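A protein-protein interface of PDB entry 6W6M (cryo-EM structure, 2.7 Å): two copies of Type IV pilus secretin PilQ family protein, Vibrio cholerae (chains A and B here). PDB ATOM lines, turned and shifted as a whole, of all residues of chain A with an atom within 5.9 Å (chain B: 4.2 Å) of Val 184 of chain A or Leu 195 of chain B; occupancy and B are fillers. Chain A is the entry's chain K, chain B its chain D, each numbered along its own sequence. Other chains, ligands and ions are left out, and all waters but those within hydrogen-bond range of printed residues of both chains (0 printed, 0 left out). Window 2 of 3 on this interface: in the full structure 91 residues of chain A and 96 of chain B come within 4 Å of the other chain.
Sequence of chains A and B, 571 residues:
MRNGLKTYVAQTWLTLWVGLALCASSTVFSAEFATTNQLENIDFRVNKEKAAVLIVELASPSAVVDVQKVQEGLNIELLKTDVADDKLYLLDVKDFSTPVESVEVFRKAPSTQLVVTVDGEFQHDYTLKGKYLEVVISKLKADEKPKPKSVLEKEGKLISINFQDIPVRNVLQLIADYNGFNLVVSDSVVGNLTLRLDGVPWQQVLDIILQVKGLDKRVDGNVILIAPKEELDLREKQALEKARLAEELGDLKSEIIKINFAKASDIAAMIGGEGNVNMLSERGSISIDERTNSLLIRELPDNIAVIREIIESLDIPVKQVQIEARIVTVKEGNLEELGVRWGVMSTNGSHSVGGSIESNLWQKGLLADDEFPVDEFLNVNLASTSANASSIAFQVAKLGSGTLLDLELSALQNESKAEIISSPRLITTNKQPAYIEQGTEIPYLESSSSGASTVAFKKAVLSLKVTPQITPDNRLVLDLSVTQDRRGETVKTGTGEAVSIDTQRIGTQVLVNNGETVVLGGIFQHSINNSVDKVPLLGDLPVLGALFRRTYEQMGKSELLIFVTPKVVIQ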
ATOM      1  N   LEU A 172      17.377  11.625  27.783  1.00  0.00           N
ATOM      2  CA  LEU A 172      16.277  10.718  27.467  1.00  0.00           C
ATOM      3  C   LEU A 172      16.787   9.441  26.815  1.00  0.00           C
ATOM      4  O   LEU A 172      16.292   8.347  27.107  1.00  0.00           O
ATOM      5  CB  LEU A 172      15.257  11.417  26.571  1.00  0.00           C
ATOM      6  CG  LEU A 172      13.973  10.617  26.342  1.00  0.00           C
ATOM      7  CD1 LEU A 172      12.789  11.558  26.198  1.00  0.00           C
ATOM      8  CD2 LEU A 172      14.092   9.722  25.122  1.00  0.00           C
ATOM      9  N   ASN A 182      12.046   1.152  25.095  1.00  0.00           N
ATOM     10  CA  ASN A 182      12.620   2.025  24.077  1.00  0.00           C
ATOM     11  C   ASN A 182      11.775   3.278  23.901  1.00  0.00           C
ATOM     12  O   ASN A 182      10.543   3.216  23.906  1.00  0.00           O
ATOM     13  CB  ASN A 182      12.733   1.270  22.752  1.00  0.00           C
ATOM     14  CG  ASN A 182      13.563   2.013  21.724  1.00  0.00           C
ATOM     15  OD1 ASN A 182      14.558   2.656  22.059  1.00  0.00           O
ATOM     16  ND2 ASN A 182      13.155   1.930  20.464  1.00  0.00           N
ATOM     17  N   LEU A 183      12.439   4.424  23.764  1.00  0.00           N
ATOM     18  CA  LEU A 183      11.754   5.694  23.585  1.00  0.00           C
ATOM     19  C   LEU A 183      12.441   6.505  22.496  1.00  0.00           C
ATOM     20  O   LEU A 183      13.641   6.363  22.252  1.00  0.00           O
ATOM     21  CB  LEU A 183      11.719   6.483  24.897  1.00  0.00           C
ATOM     22  N   VAL A 184      11.654   7.355  21.843  1.00  0.00           N
ATOM     23  CA  VAL A 184      12.121   8.191  20.746  1.00  0.00           C
ATOM     24  C   VAL A 184      11.597   9.606  20.940  1.00  0.00           C
ATOM     25  O   VAL A 184      10.591   9.829  21.622  1.00  0.00           O
ATOM     26  CB  VAL A 184      11.686   7.639  19.371  1.00  0.00           C
ATOM     27  CG1 VAL A 184      12.411   6.339  19.062  1.00  0.00           C
ATOM     28  CG2 VAL A 184      10.182   7.437  19.340  1.00  0.00           C
ATOM     29  N   VAL A 185      12.297  10.569  20.340  1.00  0.00           N
ATOM     30  CA  VAL A 185      11.951  11.980  20.475  1.00  0.00           C
ATOM     31  C   VAL A 185      11.849  12.630  19.102  1.00  0.00           C
ATOM     32  O   VAL A 185      12.147  12.004  18.079  1.00  0.00           O
ATOM     33  CB  VAL A 185      12.978  12.719  21.347  1.00  0.00           C
ATOM     34  CG1 VAL A 185      12.936  12.203  22.776  1.00  0.00           C
ATOM     35  CG2 VAL A 185      14.373  12.567  20.755  1.00  0.00           C
ATOM     36  N   SER A 186      11.438  13.894  19.075  1.00  0.00           N
ATOM     37  CA  SER A 186      11.310  14.651  17.836  1.00  0.00           C
ATOM     38  C   SER A 186      12.669  15.227  17.439  1.00  0.00           C
ATOM     39  O   SER A 186      13.714  14.865  17.988  1.00  0.00           O
ATOM     40  CB  SER A 186      10.252  15.738  17.993  1.00  0.00           C
ATOM     41  OG  SER A 186       8.967  15.174  18.193  1.00  0.00           O
ATOM     42  N   ILE A 224       7.833   4.210  23.814  1.00  0.00           N
ATOM     43  CA  ILE A 224       7.397   5.529  24.253  1.00  0.00           C
ATOM     44  C   ILE A 224       7.917   6.583  23.285  1.00  0.00           C
ATOM     45  O   ILE A 224       9.032   6.469  22.761  1.00  0.00           O
ATOM     46  CB  ILE A 224       7.868   5.818  25.692  1.00  0.00           C
ATOM     47  CG1 ILE A 224       7.543   4.629  26.599  1.00  0.00           C
ATOM     48  CG2 ILE A 224       7.213   7.081  26.227  1.00  0.00           C
ATOM     49  CD1 ILE A 224       7.789   4.888  28.070  1.00  0.00           C
ATOM     50  N   LEU A 225       7.100   7.603  23.039  1.00  0.00           N
ATOM     51  CA  LEU A 225       7.464   8.728  22.194  1.00  0.00           C
ATOM     52  C   LEU A 225       7.279  10.010  22.985  1.00  0.00           C
ATOM     53  O   LEU A 225       6.354  10.122  23.796  1.00  0.00           O
ATOM     54  CB  LEU A 225       6.620   8.757  20.908  1.00  0.00           C
ATOM     55  CG  LEU A 225       5.087   8.696  20.996  1.00  0.00           C
ATOM     56  CD1 LEU A 225       4.470  10.065  21.250  1.00  0.00           C
ATOM     57  CD2 LEU A 225       4.495   8.078  19.736  1.00  0.00           C
ATOM     58  N   ILE A 226       8.164  10.976  22.758  1.00  0.00           N
ATOM     59  CA  ILE A 226       8.131  12.248  23.470  1.00  0.00           C
ATOM     60  C   ILE A 226       7.973  13.368  22.453  1.00  0.00           C
ATOM     61  O   ILE A 226       8.494  13.281  21.336  1.00  0.00           O
ATOM     62  CB  ILE A 226       9.397  12.468  24.321  1.00  0.00           C
ATOM     63  CG1 ILE A 226      10.009  11.131  24.749  1.00  0.00           C
ATOM     64  CG2 ILE A 226       9.070  13.318  25.537  1.00  0.00           C
ATOM     65  CD1 ILE A 226       9.212  10.391  25.796  1.00  0.00           C
ATOM     66  N   ALA A 227       7.261  14.416  22.845  1.00  0.00           N
ATOM     67  CA  ALA A 227       7.046  15.575  21.990  1.00  0.00           C
ATOM     68  C   ALA A 227       6.457  16.695  22.841  1.00  0.00           C
ATOM     69  O   ALA A 227       5.940  16.439  23.935  1.00  0.00           O
ATOM     70  CB  ALA A 227       6.112  15.241  20.817  1.00  0.00           C
ATOM     71  N   ASN B 162      21.147   1.428  11.938  1.00  0.00           N
ATOM     72  CA  ASN B 162      21.764   2.550  12.645  1.00  0.00           C
ATOM     73  C   ASN B 162      22.072   3.608  11.590  1.00  0.00           C
ATOM     74  O   ASN B 162      23.071   3.495  10.872  1.00  0.00           O
ATOM     75  CB  ASN B 162      23.016   2.120  13.396  1.00  0.00           C
ATOM     76  CG  ASN B 162      23.588   3.231  14.253  1.00  0.00           C
ATOM     77  OD1 ASN B 162      23.304   4.410  14.034  1.00  0.00           O
ATOM     78  ND2 ASN B 162      24.405   2.863  15.232  1.00  0.00           N
ATOM     79  N   PHE B 163      21.211   4.620  11.496  1.00  0.00           N
ATOM     80  CA  PHE B 163      21.318   5.645  10.463  1.00  0.00           C
ATOM     81  C   PHE B 163      21.446   7.004  11.127  1.00  0.00           C
ATOM     82  O   PHE B 163      20.511   7.462  11.793  1.00  0.00           O
ATOM     83  CB  PHE B 163      20.105   5.616   9.528  1.00  0.00           C
ATOM     84  CG  PHE B 163      20.322   4.811   8.279  1.00  0.00           C
ATOM     85  CD1 PHE B 163      21.574   4.302   7.974  1.00  0.00           C
ATOM     86  CD2 PHE B 163      19.280   4.573   7.405  1.00  0.00           C
ATOM     87  CE1 PHE B 163      21.778   3.567   6.825  1.00  0.00           C
ATOM     88  CE2 PHE B 163      19.478   3.844   6.251  1.00  0.00           C
ATOM     89  CZ  PHE B 163      20.727   3.338   5.963  1.00  0.00           C
ATOM     90  N   THR B 194      18.007  10.563  12.418  1.00  0.00           N
ATOM     91  CA  THR B 194      19.073   9.775  13.020  1.00  0.00           C
ATOM     92  C   THR B 194      18.486   8.926  14.138  1.00  0.00           C
ATOM     93  O   THR B 194      17.827   9.456  15.038  1.00  0.00           O
ATOM     94  CB  THR B 194      20.190  10.678  13.557  1.00  0.00           C
ATOM     95  OG1 THR B 194      21.312   9.881  13.951  1.00  0.00           O
ATOM     96  CG2 THR B 194      19.700  11.501  14.745  1.00  0.00           C
ATOM     97  N   LEU B 195      18.725   7.617  14.074  1.00  0.00           N
ATOM     98  CA  LEU B 195      18.267   6.675  15.092  1.00  0.00           C
ATOM     99  C   LEU B 195      18.896   5.316  14.815  1.00  0.00           C
ATOM    100  O   LEU B 195      19.352   5.037  13.701  1.00  0.00           O
ATOM    101  CB  LEU B 195      16.736   6.570  15.120  1.00  0.00           C
ATOM    102  CG  LEU B 195      16.076   5.768  16.251  1.00  0.00           C
ATOM    103  CD1 LEU B 195      14.985   6.563  16.957  1.00  0.00           C
ATOM    104  CD2 LEU B 195      15.522   4.450  15.729  1.00  0.00           C
ATOM    105  N   ARG B 196      18.902   4.468  15.845  1.00  0.00           N
ATOM    106  CA  ARG B 196      19.488   3.136  15.768  1.00  0.00           C
ATOM    107  C   ARG B 196      18.644   2.153  16.565  1.00  0.00           C
ATOM    108  O   ARG B 196      18.386   2.375  17.750  1.00  0.00           O
ATOM    109  CB  ARG B 196      20.923   3.132  16.303  1.00  0.00           C
ATOM    110  CG  ARG B 196      21.029   3.451  17.787  1.00  0.00           C
ATOM    111  CD  ARG B 196      22.480   3.478  18.234  1.00  0.00           C
ATOM    112  NE  ARG B 196      22.614   3.757  19.661  1.00  0.00           N
ATOM    113  CZ  ARG B 196      22.598   2.827  20.611  1.00  0.00           C
ATOM    114  NH1 ARG B 196      22.456   1.547  20.290  1.00  0.00           N
ATOM    115  NH2 ARG B 196      22.729   3.174  21.885  1.00  0.00           N
ATOM    116  N   LEU B 197      18.238   1.064  15.912  1.00  0.00           N
ATOM    117  CA  LEU B 197      17.451   0.013  16.542  1.00  0.00           C
ATOM    118  C   LEU B 197      17.704  -1.299  15.812  1.00  0.00           C
ATOM    119  O   LEU B 197      18.217  -1.319  14.689  1.00  0.00           O
ATOM    120  CB  LEU B 197      15.951   0.339  16.539  1.00  0.00           C
ATOM    121  CG  LEU B 197      15.437   1.356  17.561  1.00  0.00           C
ATOM    122  CD1 LEU B 197      13.950   1.603  17.369  1.00  0.00           C
ATOM    123  CD2 LEU B 197      15.736   0.886  18.980  1.00  0.00           C
ATOM    124  N   ILE B 208       6.358   4.167  14.778  1.00  0.00           N
ATOM    125  CA  ILE B 208       6.872   5.174  15.700  1.00  0.00           C
ATOM    126  C   ILE B 208       7.608   6.268  14.932  1.00  0.00           C
ATOM    127  O   ILE B 208       7.516   7.456  15.285  1.00  0.00           O
ATOM    128  CB  ILE B 208       7.751   4.520  16.786  1.00  0.00           C
ATOM    129  CG1 ILE B 208       7.870   5.435  18.005  1.00  0.00           C
ATOM    130  CG2 ILE B 208       9.135   4.166  16.263  1.00  0.00           C
ATOM    131  CD1 ILE B 208       6.630   5.473  18.864  1.00  0.00           C
ATOM    132  N   VAL B 212       6.248  10.151  15.226  1.00  0.00           N
ATOM    133  CA  VAL B 212       7.016  11.204  15.886  1.00  0.00           C
ATOM    134  C   VAL B 212       7.389  12.300  14.893  1.00  0.00           C
ATOM    135  O   VAL B 212       6.999  13.462  15.053  1.00  0.00           O
ATOM    136  CB  VAL B 212       8.254  10.614  16.576  1.00  0.00           C
ATOM    137  CG1 VAL B 212       9.119  11.724  17.147  1.00  0.00           C
ATOM    138  CG2 VAL B 212       7.821   9.656  17.672  1.00  0.00           C
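Hydrophobic or aromatic side chains of chain A within 4 Å of the printed part of chain B: Val 184 and Leu 225. Among the printed residues, 8 pairs touch across the chains.
No position is printed for both chains. Of the 8 pairs that touch across the chains among the printed residues, none has its exchanged pair printed and touching as well.
Among the printed residues, pairs that only touch across the chains: Asn 182 of chain A with Leu 197 of chain B (3.2 Å), Val 185 of chain A with Val 212 of chain B (3.2 Å), Val 184 of chain A with Leu 195 of chain B (3.3 Å), Val 184 of chain A with Ile 208 of chain B (3.3 Å), Leu 225 of chain A with Ile 208 of chain B (3.5 Å), Leu 225 of chain A with Val 212 of chain B (3.6 Å), Ser 186 of chain A with Val 212 of chain B (3.6 Å) and Val 184 of chain A with Val 212 of chain B (3.6 Å).
Val 184 of chain A touches three residues of chain B. Printed residues of chain A within 4 Å of Leu 195 of chain B: Val 184. Of the printed residues of chain A, Val 212 of chain B touches Val 184, Val 185, Ser 186 and Leu 225. Printed residues of chain B within 4 Å of Val 185 of chain A: Val 212. Printed residues of chain A within 4 Å of Ile 208 of chain B: Val 184 (3.3 Å) and Leu 225 (3.5 Å). Of the printed residues of chain B, Ser 186 of chain A touches Val 212. Of the printed residues of chain B, Leu 225 of chain A touches Ile 208 and Val 212. Phe 163 of chain B touches none of the printed residues of chain A. The nearest printed residue of chain B that does not touch Val 184 of chain A is Leu 197 of chain B (5.3 Å).
O of Asn 182 of chain A is in hydrogen-bond range of N of Ile 224 of chain A. The backbone NH of Leu 195 of chain B sits at hydrogen-bond distance from the backbone carbonyl oxygen of Phe 163 of chain B (2.9 Å). N of Val 184 of chain A sits at hydrogen-bond distance from O of Ile 224 of chain A, at 2.9 Å. N of Ile 226 of chain A sits at hydrogen-bond distance from O of Val 184 of chain A.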
